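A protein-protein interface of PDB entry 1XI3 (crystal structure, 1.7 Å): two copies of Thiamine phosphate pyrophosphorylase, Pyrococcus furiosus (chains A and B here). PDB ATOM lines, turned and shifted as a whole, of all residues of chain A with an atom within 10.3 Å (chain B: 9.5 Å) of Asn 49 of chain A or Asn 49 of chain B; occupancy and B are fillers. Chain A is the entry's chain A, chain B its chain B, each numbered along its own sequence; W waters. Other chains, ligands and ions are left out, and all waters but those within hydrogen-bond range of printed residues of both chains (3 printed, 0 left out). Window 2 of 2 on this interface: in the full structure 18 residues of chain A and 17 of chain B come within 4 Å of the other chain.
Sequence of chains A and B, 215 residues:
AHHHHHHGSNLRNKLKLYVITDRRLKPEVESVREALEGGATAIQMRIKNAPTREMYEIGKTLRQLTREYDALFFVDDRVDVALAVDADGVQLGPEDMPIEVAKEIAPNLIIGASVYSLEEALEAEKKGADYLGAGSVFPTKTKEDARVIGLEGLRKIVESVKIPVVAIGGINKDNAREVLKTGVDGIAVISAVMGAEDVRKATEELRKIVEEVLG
OD2 of Asp 77 of chain A is in hydrogen-bond range of OG1 of Thr 52 of chain B, at 2.8 Å. OG1 of Thr 52 of chain A lies within hydrogen-bond range of OD1 of Asp 77 of chain B, at 2.8 Å. N of Arg 53 of chain A sits at hydrogen-bond distance from O of Glu 95 of chain B, at 2.9 Å. NE of Arg 78 of chain A lies close to NE of Arg 78 of chain B (3.3 Å). ND2 of Asn 49 of chain B lies close to ND2 of Asn 49 of chain A (3.4 Å). The backbone carbonyl oxygen (O) of Glu 95 of chain B lies within hydrogen-bond range of the backbone NH (N) of Thr 52 of chain A, at 3.4 Å. N of Thr 52 of chain B sits at hydrogen-bond distance from O of Glu 95 of chain A (3.4 Å).
NH1 of Arg 78 of chain A lies within hydrogen-bond range of SD of Met 55 of chain A, 3.5 Å away. NH1 of Arg 78 of chain B sits at hydrogen-bond distance from SD of Met 55 of chain B, 3.5 Å away. OG1 of Thr 52 of chain A is in hydrogen-bond range of NH2 of Arg 78 of chain A (2.9 Å). NH2 of Arg 78 of chain B is in hydrogen-bond range of OG1 of Thr 52 of chain B (2.9 Å).
Among the printed residues, merely in contact across the chains: Pro 51 of chain A with Glu 95 of chain B (3.3 Å) and Glu 95 of chain A with Pro 51 of chain B (3.5 Å).
Arg 23 of chain A touches none of the printed residues of chain B. No residue of chain B comes within 4 Å of Lys 48 of chain A. Of the printed residues of chain B, Asn 49 of chain A touches Asn 49. No residue of chain B comes within 4 Å of Ala 50 of chain A. Ile 47 of chain B touches none of the printed residues of chain A. No residue of chain A comes within 4 Å of Lys 48 of chain B. Asn 49 of chain B touches one residue of chain A. No residue of chain A comes within 4 Å of Ala 50 of chain B. Of the printed residues of chain A, Thr 52 of chain B touches Asp 77 (2.8 Å) and Glu 95 (3.4 Å). Of the printed residues of chain A, Glu 95 of chain B touches Pro 51 (3.3 Å), Thr 52 (3.4 Å) and Arg 53 (2.9 Å). The nearest residue of chain B that does not touch Asn 49 of chain A is Lys 48 of chain B (6.6 Å). The nearest residue of chain A that does not touch Asn 49 of chain B is Ala 50 of chain A (7.2 Å). The nearest printed residue of chain B that does not touch Glu 95 of chain A is Glu 54 of chain B (4.9 Å).
Of the 17 printed residues of chain B, 6 touch a printed residue of chain A. Hydrophobic or aromatic side chains of chain B within 4 Å of the printed part of chain A: Pro 51. Among the printed residues, 9 pairs touch across the chains. Among the printed residues, no Asp or Glu carboxylate lies within 4 Å of a Lys or Arg side-chain nitrogen of the other chain.
Pro 51 of chain A touches Glu 95 of chain B, and with the chains exchanged Glu 95 of chain A touches Pro 51 of chain B. Thr 52 of chain A touches Asp 77 of chain B, and with the chains exchanged Asp 77 of chain A touches Thr 52 of chain B. Thr 52 of chain A touches Glu 95 of chain B, and with the chains exchanged Glu 95 of chain A touches Thr 52 of chain B. Arg 78 of chain B touches its own counterpart, Arg 78 of chain A.
Water W1 lies within hydrogen-bond range of the side-chain carboxylate of Asp 77 of chain B (2.7 Å), the backbone NH of Thr 52 of chain A (2.9 Å) and the backbone carbonyl oxygen of Glu 95 of chain B (3.0 Å). Water W3 lies within hydrogen-bond range of OD1 of Asp 77 of chain A (2.8 Å), N of Thr 52 of chain B (2.9 Å) and O of Glu 95 of chain A (3.1 Å).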
ATOM      1  N   ARG A  23      27.240  11.057  36.982  1.00  0.00           N
ATOM      2  CA  ARG A  23      27.589   9.682  36.614  1.00  0.00           C
ATOM      3  C   ARG A  23      29.106   9.468  36.492  1.00  0.00           C
ATOM      4  O   ARG A  23      29.557   8.316  36.395  1.00  0.00           O
ATOM      5  CB  ARG A  23      26.889   9.281  35.319  1.00  0.00           C
ATOM      6  CG  ARG A  23      27.255  10.158  34.127  1.00  0.00           C
ATOM      7  CD  ARG A  23      26.682   9.655  32.802  1.00  0.00           C
ATOM      8  NE  ARG A  23      25.263   9.334  32.886  1.00  0.00           N
ATOM      9  CZ  ARG A  23      24.572   8.707  31.944  1.00  0.00           C
ATOM     10  NH1 ARG A  23      25.148   8.346  30.794  1.00  0.00           N
ATOM     11  NH2 ARG A  23      23.298   8.434  32.166  1.00  0.00           N
ATOM     12  N   ARG A  24      29.879  10.554  36.462  1.00  0.00           N
ATOM     13  CA  ARG A  24      31.356  10.423  36.590  1.00  0.00           C
ATOM     14  C   ARG A  24      31.769   9.825  37.939  1.00  0.00           C
ATOM     15  O   ARG A  24      32.868   9.206  38.052  1.00  0.00           O
ATOM     16  CB  ARG A  24      32.081  11.739  36.348  1.00  0.00           C
ATOM     17  CG  ARG A  24      31.889  12.315  34.960  1.00  0.00           C
ATOM     18  CD  ARG A  24      32.457  13.708  34.827  1.00  0.00           C
ATOM     19  NE  ARG A  24      31.758  14.629  35.720  1.00  0.00           N
ATOM     20  CZ  ARG A  24      31.948  15.937  35.763  1.00  0.00           C
ATOM     21  NH1 ARG A  24      32.802  16.519  34.937  1.00  0.00           N
ATOM     22  NH2 ARG A  24      31.243  16.677  36.616  1.00  0.00           N
ATOM     23  N   GLU A  28      23.150   7.255  38.332  1.00  0.00           N
ATOM     24  CA  GLU A  28      22.115   8.175  38.800  1.00  0.00           C
ATOM     25  C   GLU A  28      21.037   7.493  39.641  1.00  0.00           C
ATOM     26  O   GLU A  28      20.682   7.980  40.718  1.00  0.00           O
ATOM     27  CB  GLU A  28      21.463   8.866  37.610  1.00  0.00           C
ATOM     28  CG  GLU A  28      22.317   9.918  36.901  1.00  0.00           C
ATOM     29  CD  GLU A  28      22.963   9.451  35.620  1.00  0.00           C
ATOM     30  OE1 GLU A  28      22.774   8.287  35.228  1.00  0.00           O
ATOM     31  OE2 GLU A  28      23.681  10.291  34.999  1.00  0.00           O
ATOM     32  N   ARG A  46      21.611  15.711  35.901  1.00  0.00           N
ATOM     33  CA  ARG A  46      22.553  16.494  35.085  1.00  0.00           C
ATOM     34  C   ARG A  46      23.416  15.483  34.330  1.00  0.00           C
ATOM     35  O   ARG A  46      24.346  14.894  34.903  1.00  0.00           O
ATOM     36  CB  ARG A  46      23.398  17.410  35.974  1.00  0.00           C
ATOM     37  CG  ARG A  46      24.397  18.254  35.218  1.00  0.00           C
ATOM     38  CD  ARG A  46      25.156  19.177  36.111  1.00  0.00           C
ATOM     39  NE  ARG A  46      26.145  19.871  35.303  1.00  0.00           N
ATOM     40  CZ  ARG A  46      27.363  19.408  35.021  1.00  0.00           C
ATOM     41  NH1 ARG A  46      27.769  18.225  35.489  1.00  0.00           N
ATOM     42  NH2 ARG A  46      28.192  20.141  34.259  1.00  0.00           N
ATOM     43  N   ILE A  47      23.072  15.257  33.063  1.00  0.00           N
ATOM     44  CA  ILE A  47      23.754  14.268  32.210  1.00  0.00           C
ATOM     45  C   ILE A  47      24.352  14.966  30.972  1.00  0.00           C
ATOM     46  O   ILE A  47      23.635  15.619  30.235  1.00  0.00           O
ATOM     47  CB  ILE A  47      22.795  13.217  31.747  1.00  0.00           C
ATOM     48  CG1 ILE A  47      22.171  12.484  32.950  1.00  0.00           C
ATOM     49  CG2 ILE A  47      23.488  12.234  30.866  1.00  0.00           C
ATOM     50  CD1 ILE A  47      21.086  11.566  32.576  1.00  0.00           C
ATOM     51  N   LYS A  48      25.651  14.820  30.789  1.00  0.00           N
ATOM     52  CA  LYS A  48      26.359  15.284  29.566  1.00  0.00           C
ATOM     53  C   LYS A  48      26.570  14.101  28.622  1.00  0.00           C
ATOM     54  O   LYS A  48      26.908  13.011  29.063  1.00  0.00           O
ATOM     55  CB  LYS A  48      27.719  15.834  29.969  1.00  0.00           C
ATOM     56  N   ASN A  49      26.368  14.321  27.330  1.00  0.00           N
ATOM     57  CA  ASN A  49      26.774  13.372  26.305  1.00  0.00           C
ATOM     58  C   ASN A  49      26.147  11.991  26.443  1.00  0.00           C
ATOM     59  O   ASN A  49      26.855  10.969  26.426  1.00  0.00           O
ATOM     60  CB  ASN A  49      28.303  13.244  26.286  1.00  0.00           C
ATOM     61  CG  ASN A  49      28.993  14.577  26.113  1.00  0.00           C
ATOM     62  OD1 ASN A  49      29.772  15.013  26.982  1.00  0.00           O
ATOM     63  ND2 ASN A  49      28.706  15.247  25.005  1.00  0.00           N
ATOM     64  N   ALA A  50      24.828  11.959  26.605  1.00  0.00           N
ATOM     65  CA  ALA A  50      24.049  10.736  26.443  1.00  0.00           C
ATOM     66  C   ALA A  50      22.918  10.999  25.454  1.00  0.00           C
ATOM     67  O   ALA A  50      22.439  12.118  25.350  1.00  0.00           O
ATOM     68  CB  ALA A  50      23.468  10.312  27.744  1.00  0.00           C
ATOM     69  N   PRO A  51      22.463   9.955  24.770  1.00  0.00           N
ATOM     70  CA  PRO A  51      21.333  10.072  23.836  1.00  0.00           C
ATOM     71  C   PRO A  51      20.067  10.516  24.562  1.00  0.00           C
ATOM     72  O   PRO A  51      19.881  10.226  25.742  1.00  0.00           O
ATOM     73  CB  PRO A  51      21.157   8.652  23.271  1.00  0.00           C
ATOM     74  CG  PRO A  51      22.036   7.791  23.997  1.00  0.00           C
ATOM     75  CD  PRO A  51      23.010   8.593  24.815  1.00  0.00           C
ATOM     76  N   THR A  52      19.209  11.225  23.852  1.00  0.00           N
ATOM     77  CA  THR A  52      17.973  11.679  24.419  1.00  0.00           C
ATOM     78  C   THR A  52      17.132  10.537  24.972  1.00  0.00           C
ATOM     79  O   THR A  52      16.522  10.662  26.035  1.00  0.00           O
ATOM     80  CB  THR A  52      17.200  12.475  23.381  1.00  0.00           C
ATOM     81  OG1 THR A  52      18.008  13.563  22.945  1.00  0.00           O
ATOM     82  CG2 THR A  52      15.923  12.996  23.954  1.00  0.00           C
ATOM     83  N   ARG A  53      17.167   9.393  24.300  1.00  0.00           N
ATOM     84  CA  ARG A  53      16.403   8.230  24.766  1.00  0.00           C
ATOM     85  C   ARG A  53      16.818   7.828  26.183  1.00  0.00           C
ATOM     86  O   ARG A  53      15.982   7.551  27.033  1.00  0.00           O
ATOM     87  CB  ARG A  53      16.563   7.039  23.838  1.00  0.00           C
ATOM     88  CG  ARG A  53      15.762   5.834  24.290  1.00  0.00           C
ATOM     89  CD  ARG A  53      15.809   4.766  23.243  1.00  0.00           C
ATOM     90  NE  ARG A  53      14.483   4.198  23.121  1.00  0.00           N
ATOM     91  CZ  ARG A  53      13.503   4.641  22.337  1.00  0.00           C
ATOM     92  NH1 ARG A  53      12.365   4.017  22.430  1.00  0.00           N
ATOM     93  NH2 ARG A  53      13.628   5.689  21.477  1.00  0.00           N
ATOM     94  N   GLU A  54      18.113   7.818  26.419  1.00  0.00           N
ATOM     95  CA  GLU A  54      18.665   7.459  27.713  1.00  0.00           C
ATOM     96  C   GLU A  54      18.311   8.465  28.789  1.00  0.00           C
ATOM     97  O   GLU A  54      17.910   8.116  29.919  1.00  0.00           O
ATOM     98  CB  GLU A  54      20.181   7.340  27.589  1.00  0.00           C
ATOM     99  CG  GLU A  54      20.842   6.990  28.931  1.00  0.00           C
ATOM    100  CD  GLU A  54      22.288   6.703  28.841  1.00  0.00           C
ATOM    101  OE1 GLU A  54      22.816   6.489  27.705  1.00  0.00           O
ATOM    102  OE2 GLU A  54      22.911   6.655  29.931  1.00  0.00           O
ATOM    103  N   MET A  55      18.475   9.753  28.455  1.00  0.00           N
ATOM    104  CA  MET A  55      18.055  10.827  29.373  1.00  0.00           C
ATOM    105  C   MET A  55      16.572  10.672  29.770  1.00  0.00           C
ATOM    106  O   MET A  55      16.204  10.821  30.938  1.00  0.00           O
ATOM    107  CB  MET A  55      18.301  12.192  28.728  1.00  0.00           C
ATOM    108  CG  MET A  55      19.766  12.454  28.420  1.00  0.00           C
ATOM    109  SD  MET A  55      19.886  14.111  27.758  1.00  0.00           S
ATOM    110  CE  MET A  55      21.628  14.395  27.700  1.00  0.00           C
ATOM    111  N   ILE A  58      16.120   7.361  32.115  1.00  0.00           N
ATOM    112  CA  ILE A  58      16.615   7.646  33.476  1.00  0.00           C
ATOM    113  C   ILE A  58      15.695   8.692  34.153  1.00  0.00           C
ATOM    114  O   ILE A  58      15.356   8.607  35.356  1.00  0.00           O
ATOM    115  CB  ILE A  58      18.088   8.088  33.433  1.00  0.00           C
ATOM    116  CG1 ILE A  58      18.960   6.935  32.911  1.00  0.00           C
ATOM    117  CG2 ILE A  58      18.548   8.548  34.843  1.00  0.00           C
ATOM    118  CD1 ILE A  58      20.392   7.316  32.753  1.00  0.00           C
ATOM    119  N   ASP A  76      18.862  19.477  34.388  1.00  0.00           N
ATOM    120  CA  ASP A  76      19.812  20.512  33.943  1.00  0.00           C
ATOM    121  C   ASP A  76      19.686  20.690  32.426  1.00  0.00           C
ATOM    122  O   ASP A  76      19.699  19.683  31.701  1.00  0.00           O
ATOM    123  CB  ASP A  76      21.236  20.135  34.272  1.00  0.00           C
ATOM    124  CG  ASP A  76      22.194  21.272  33.996  1.00  0.00           C
ATOM    125  OD1 ASP A  76      23.199  21.011  33.337  1.00  0.00           O
ATOM    126  OD2 ASP A  76      21.896  22.401  34.407  1.00  0.00           O
ATOM    127  N   ASP A  77      19.502  21.951  31.985  1.00  0.00           N
ATOM    128  CA  ASP A  77      19.543  22.352  30.552  1.00  0.00           C
ATOM    129  C   ASP A  77      18.294  21.937  29.795  1.00  0.00           C
ATOM    130  O   ASP A  77      17.532  22.788  29.311  1.00  0.00           O
ATOM    131  CB  ASP A  77      20.833  21.734  29.947  1.00  0.00           C
ATOM    132  CG  ASP A  77      21.115  22.083  28.487  1.00  0.00           C
ATOM    133  OD1 ASP A  77      22.260  21.722  28.049  1.00  0.00           O
ATOM    134  OD2 ASP A  77      20.283  22.633  27.762  1.00  0.00           O
ATOM    135  N   ARG A  78      18.076  20.634  29.708  1.00  0.00           N
ATOM    136  CA  ARG A  78      17.210  20.047  28.680  1.00  0.00           C
ATOM    137  C   ARG A  78      15.719  20.163  28.980  1.00  0.00           C
ATOM    138  O   ARG A  78      15.146  19.337  29.711  1.00  0.00           O
ATOM    139  CB  ARG A  78      17.630  18.552  28.410  1.00  0.00           C
ATOM    140  CG  ARG A  78      19.033  18.411  27.856  1.00  0.00           C
ATOM    141  CD  ARG A  78      19.049  18.863  26.384  1.00  0.00           C
ATOM    142  NE  ARG A  78      18.245  17.965  25.586  1.00  0.00           N
ATOM    143  CZ  ARG A  78      18.704  16.832  25.050  1.00  0.00           C
ATOM    144  NH1 ARG A  78      19.954  16.486  25.178  1.00  0.00           N
ATOM    145  NH2 ARG A  78      17.891  16.053  24.397  1.00  0.00           N
ATOM    146  N   GLU A  95      24.820  28.957  28.667  1.00  0.00           N
ATOM    147  CA  GLU A  95      24.893  28.186  27.393  1.00  0.00           C
ATOM    148  C   GLU A  95      23.595  27.457  27.063  1.00  0.00           C
ATOM    149  O   GLU A  95      23.547  26.667  26.120  1.00  0.00           O
ATOM    150  CB  GLU A  95      26.036  27.185  27.462  1.00  0.00           C
ATOM    151  CG  GLU A  95      27.418  27.863  27.658  1.00  0.00           C
ATOM    152  N   ARG B  23      27.922  20.580   9.681  1.00  0.00           N
ATOM    153  CA  ARG B  23      28.948  21.577   9.953  1.00  0.00           C
ATOM    154  C   ARG B  23      30.366  20.989   9.804  1.00  0.00           C
ATOM    155  O   ARG B  23      31.310  21.763   9.770  1.00  0.00           O
ATOM    156  CB  ARG B  23      28.808  22.207  11.328  1.00  0.00           C
ATOM    157  CG  ARG B  23      28.701  21.252  12.467  1.00  0.00           C
ATOM    158  CD  ARG B  23      28.822  21.982  13.798  1.00  0.00           C
ATOM    159  NE  ARG B  23      27.780  22.971  13.960  1.00  0.00           N
ATOM    160  CZ  ARG B  23      27.704  23.843  14.964  1.00  0.00           C
ATOM    161  NH1 ARG B  23      26.728  24.753  14.968  1.00  0.00           N
ATOM    162  NH2 ARG B  23      28.600  23.815  15.944  1.00  0.00           N
ATOM    163  N   ARG B  24      30.509  19.670   9.753  1.00  0.00           N
ATOM    164  CA  ARG B  24      31.835  19.075   9.422  1.00  0.00           C
ATOM    165  C   ARG B  24      32.204  19.465   7.999  1.00  0.00           C
ATOM    166  O   ARG B  24      33.388  19.506   7.629  1.00  0.00           O
ATOM    167  CB  ARG B  24      31.831  17.561   9.560  1.00  0.00           C
ATOM    168  CG  ARG B  24      31.765  17.084  11.008  1.00  0.00           C
ATOM    169  CD  ARG B  24      31.637  15.581  11.106  1.00  0.00           C
ATOM    170  NE  ARG B  24      30.256  15.082  11.068  1.00  0.00           N
ATOM    171  CZ  ARG B  24      29.732  14.338  10.089  1.00  0.00           C
ATOM    172  NH1 ARG B  24      30.452  14.005   9.019  1.00  0.00           N
ATOM    173  NH2 ARG B  24      28.460  13.925  10.174  1.00  0.00           N
ATOM    174  N   GLU B  28      26.385  26.007   8.780  1.00  0.00           N
ATOM    175  CA  GLU B  28      24.943  25.805   8.507  1.00  0.00           C
ATOM    176  C   GLU B  28      24.257  26.915   7.773  1.00  0.00           C
ATOM    177  O   GLU B  28      23.537  26.664   6.826  1.00  0.00           O
ATOM    178  CB  GLU B  28      24.224  25.573   9.818  1.00  0.00           C
ATOM    179  CG  GLU B  28      24.503  24.200  10.439  1.00  0.00           C
ATOM    180  CD  GLU B  28      25.483  24.215  11.594  1.00  0.00           C
ATOM    181  OE1 GLU B  28      25.734  23.131  12.169  1.00  0.00           O
ATOM    182  OE2 GLU B  28      26.061  25.277  11.907  1.00  0.00           O
ATOM    183  N   ARG B  46      20.941  19.623  11.801  1.00  0.00           N
ATOM    184  CA  ARG B  46      21.446  18.460  12.501  1.00  0.00           C
ATOM    185  C   ARG B  46      22.791  18.829  13.106  1.00  0.00           C
ATOM    186  O   ARG B  46      23.788  18.884  12.402  1.00  0.00           O
ATOM    187  CB  ARG B  46      21.536  17.254  11.570  1.00  0.00           C
ATOM    188  CG  ARG B  46      22.114  15.977  12.239  1.00  0.00           C
ATOM    189  CD  ARG B  46      21.915  14.726  11.365  1.00  0.00           C
ATOM    190  NE  ARG B  46      22.662  13.557  11.856  1.00  0.00           N
ATOM    191  CZ  ARG B  46      22.161  12.372  12.218  1.00  0.00           C
ATOM    192  NH1 ARG B  46      20.848  12.117  12.212  1.00  0.00           N
ATOM    193  NH2 ARG B  46      23.005  11.413  12.607  1.00  0.00           N
ATOM    194  N   ILE B  47      22.799  19.102  14.416  1.00  0.00           N
ATOM    195  CA  ILE B  47      24.024  19.573  15.080  1.00  0.00           C
ATOM    196  C   ILE B  47      24.299  18.552  16.192  1.00  0.00           C
ATOM    197  O   ILE B  47      23.454  18.356  17.074  1.00  0.00           O
ATOM    198  CB  ILE B  47      23.867  20.974  15.644  1.00  0.00           C
ATOM    199  CG1 ILE B  47      23.618  21.994  14.537  1.00  0.00           C
ATOM    200  CG2 ILE B  47      25.104  21.379  16.409  1.00  0.00           C
ATOM    201  CD1 ILE B  47      23.204  23.354  15.028  1.00  0.00           C
ATOM    202  N   LYS B  48      25.457  17.902  16.098  1.00  0.00           N
ATOM    203  CA  LYS B  48      25.786  16.740  16.950  1.00  0.00           C
ATOM    204  C   LYS B  48      26.055  17.130  18.395  1.00  0.00           C
ATOM    205  O   LYS B  48      25.516  16.490  19.319  1.00  0.00           O
ATOM    206  CB  LYS B  48      27.012  16.026  16.406  1.00  0.00           C
ATOM    207  N   ASN B  49      26.901  18.145  18.590  1.00  0.00           N
ATOM    208  CA  ASN B  49      27.434  18.481  19.916  1.00  0.00           C
ATOM    209  C   ASN B  49      27.709  19.966  20.017  1.00  0.00           C
ATOM    210  O   ASN B  49      28.826  20.418  19.767  1.00  0.00           O
ATOM    211  CB  ASN B  49      28.773  17.790  20.176  1.00  0.00           C
ATOM    212  CG  ASN B  49      28.639  16.332  20.546  1.00  0.00           C
ATOM    213  OD1 ASN B  49      28.974  15.448  19.755  1.00  0.00           O
ATOM    214  ND2 ASN B  49      28.191  16.069  21.771  1.00  0.00           N
ATOM    215  N   ALA B  50      26.720  20.728  20.431  1.00  0.00           N
ATOM    216  CA  ALA B  50      26.877  22.164  20.588  1.00  0.00           C
ATOM    217  C   ALA B  50      25.954  22.554  21.741  1.00  0.00           C
ATOM    218  O   ALA B  50      24.950  21.872  21.971  1.00  0.00           O
ATOM    219  CB  ALA B  50      26.487  22.896  19.331  1.00  0.00           C
ATOM    220  N   PRO B  51      26.256  23.657  22.412  1.00  0.00           N
ATOM    221  CA  PRO B  51      25.368  24.091  23.494  1.00  0.00           C
ATOM    222  C   PRO B  51      23.968  24.389  22.996  1.00  0.00           C
ATOM    223  O   PRO B  51      23.766  24.816  21.855  1.00  0.00           O
ATOM    224  CB  PRO B  51      26.011  25.356  24.038  1.00  0.00           C
ATOM    225  CG  PRO B  51      27.279  25.538  23.347  1.00  0.00           C
ATOM    226  CD  PRO B  51      27.406  24.545  22.235  1.00  0.00           C
ATOM    227  N   THR B  52      22.989  24.174  23.852  1.00  0.00           N
ATOM    228  CA  THR B  52      21.615  24.498  23.481  1.00  0.00           C
ATOM    229  C   THR B  52      21.439  25.945  22.971  1.00  0.00           C
ATOM    230  O   THR B  52      20.692  26.184  22.016  1.00  0.00           O
ATOM    231  CB  THR B  52      20.660  24.172  24.653  1.00  0.00           C
ATOM    232  OG1 THR B  52      20.835  22.793  25.007  1.00  0.00           O
ATOM    233  CG2 THR B  52      19.245  24.401  24.270  1.00  0.00           C
ATOM    234  N   GLU B  54      23.422  27.801  21.344  1.00  0.00           N
ATOM    235  CA  GLU B  54      23.935  27.888  19.972  1.00  0.00           C
ATOM    236  C   GLU B  54      22.969  27.248  18.982  1.00  0.00           C
ATOM    237  O   GLU B  54      22.714  27.772  17.902  1.00  0.00           O
ATOM    238  CB  GLU B  54      25.305  27.238  19.888  1.00  0.00           C
ATOM    239  CG  GLU B  54      25.910  27.275  18.459  1.00  0.00           C
ATOM    240  CD  GLU B  54      27.218  26.591  18.356  1.00  0.00           C
ATOM    241  OE1 GLU B  54      27.885  26.382  19.387  1.00  0.00           O
ATOM    242  OE2 GLU B  54      27.641  26.300  17.206  1.00  0.00           O
ATOM    243  N   MET B  55      22.432  26.082  19.345  1.00  0.00           N
ATOM    244  CA  MET B  55      21.441  25.423  18.496  1.00  0.00           C
ATOM    245  C   MET B  55      20.233  26.328  18.288  1.00  0.00           C
ATOM    246  O   MET B  55      19.642  26.405  17.179  1.00  0.00           O
ATOM    247  CB  MET B  55      21.012  24.086  19.137  1.00  0.00           C
ATOM    248  CG  MET B  55      22.102  23.088  19.213  1.00  0.00           C
ATOM    249  SD  MET B  55      21.460  21.576  19.988  1.00  0.00           S
ATOM    250  CE  MET B  55      22.937  20.536  19.889  1.00  0.00           C
ATOM    251  N   ILE B  58      21.283  29.420  15.868  1.00  0.00           N
ATOM    252  CA  ILE B  58      21.365  28.966  14.472  1.00  0.00           C
ATOM    253  C   ILE B  58      19.972  28.603  13.981  1.00  0.00           C
ATOM    254  O   ILE B  58      19.557  28.959  12.845  1.00  0.00           O
ATOM    255  CB  ILE B  58      22.340  27.807  14.335  1.00  0.00           C
ATOM    256  CG1 ILE B  58      23.744  28.279  14.734  1.00  0.00           C
ATOM    257  CG2 ILE B  58      22.313  27.240  12.923  1.00  0.00           C
ATOM    258  CD1 ILE B  58      24.726  27.206  14.758  1.00  0.00           C
ATOM    259  N   ASP B  76      16.838  17.769  13.779  1.00  0.00           N
ATOM    260  CA  ASP B  76      17.138  16.397  14.189  1.00  0.00           C
ATOM    261  C   ASP B  76      17.134  16.295  15.706  1.00  0.00           C
ATOM    262  O   ASP B  76      17.789  17.111  16.385  1.00  0.00           O
ATOM    263  CB  ASP B  76      18.518  15.956  13.685  1.00  0.00           C
ATOM    264  CG  ASP B  76      18.735  14.448  13.823  1.00  0.00           C
ATOM    265  OD1 ASP B  76      17.818  13.668  13.514  1.00  0.00           O
ATOM    266  OD2 ASP B  76      19.845  14.057  14.257  1.00  0.00           O
ATOM    267  N   ASP B  77      16.411  15.281  16.221  1.00  0.00           N
ATOM    268  CA  ASP B  77      16.449  14.867  17.635  1.00  0.00           C
ATOM    269  C   ASP B  77      15.719  15.867  18.535  1.00  0.00           C
ATOM    270  O   ASP B  77      14.681  15.541  19.123  1.00  0.00           O
ATOM    271  CB  ASP B  77      17.915  14.601  18.039  1.00  0.00           C
ATOM    272  CG  ASP B  77      18.137  14.168  19.500  1.00  0.00           C
ATOM    273  OD1 ASP B  77      17.232  14.124  20.354  1.00  0.00           O
ATOM    274  OD2 ASP B  77      19.342  13.861  19.749  1.00  0.00           O
ATOM    275  N   ARG B  78      16.195  17.112  18.571  1.00  0.00           N
ATOM    276  CA  ARG B  78      15.939  18.013  19.687  1.00  0.00           C
ATOM    277  C   ARG B  78      14.576  18.723  19.618  1.00  0.00           C
ATOM    278  O   ARG B  78      14.380  19.761  18.957  1.00  0.00           O
ATOM    279  CB  ARG B  78      17.093  19.013  19.805  1.00  0.00           C
ATOM    280  CG  ARG B  78      18.438  18.404  20.150  1.00  0.00           C
ATOM    281  CD  ARG B  78      18.489  17.940  21.606  1.00  0.00           C
ATOM    282  NE  ARG B  78      18.338  19.085  22.482  1.00  0.00           N
ATOM    283  CZ  ARG B  78      19.355  19.809  22.953  1.00  0.00           C
ATOM    284  NH1 ARG B  78      20.610  19.470  22.701  1.00  0.00           N
ATOM    285  NH2 ARG B  78      19.104  20.851  23.678  1.00  0.00           N
ATOM    286  N   GLU B  95      17.607   6.450  18.987  1.00  0.00           N
ATOM    287  CA  GLU B  95      18.289   6.983  20.179  1.00  0.00           C
ATOM    288  C   GLU B  95      17.668   8.265  20.702  1.00  0.00           C
ATOM    289  O   GLU B  95      18.232   8.932  21.599  1.00  0.00           O
ATOM    290  CB  GLU B  95      19.774   7.179  19.872  1.00  0.00           C
ATOM    291  CG  GLU B  95      20.507   5.842  19.769  1.00  0.00           C
ATOM    292  CD  GLU B  95      20.503   5.097  21.079  1.00  0.00           C
ATOM    293  OE1 GLU B  95      19.608   4.259  21.309  1.00  0.00           O
ATOM    294  OE2 GLU B  95      21.386   5.382  21.899  1.00  0.00           O
HETATM  295  O   HOH W   1      19.737  11.487  20.988  1.00  0.00           O
HETATM  296  O   HOH W   2      23.016  20.308  25.949  1.00  0.00           O
HETATM  297  O   HOH W   3      23.668  23.654  26.607  1.00  0.00           O
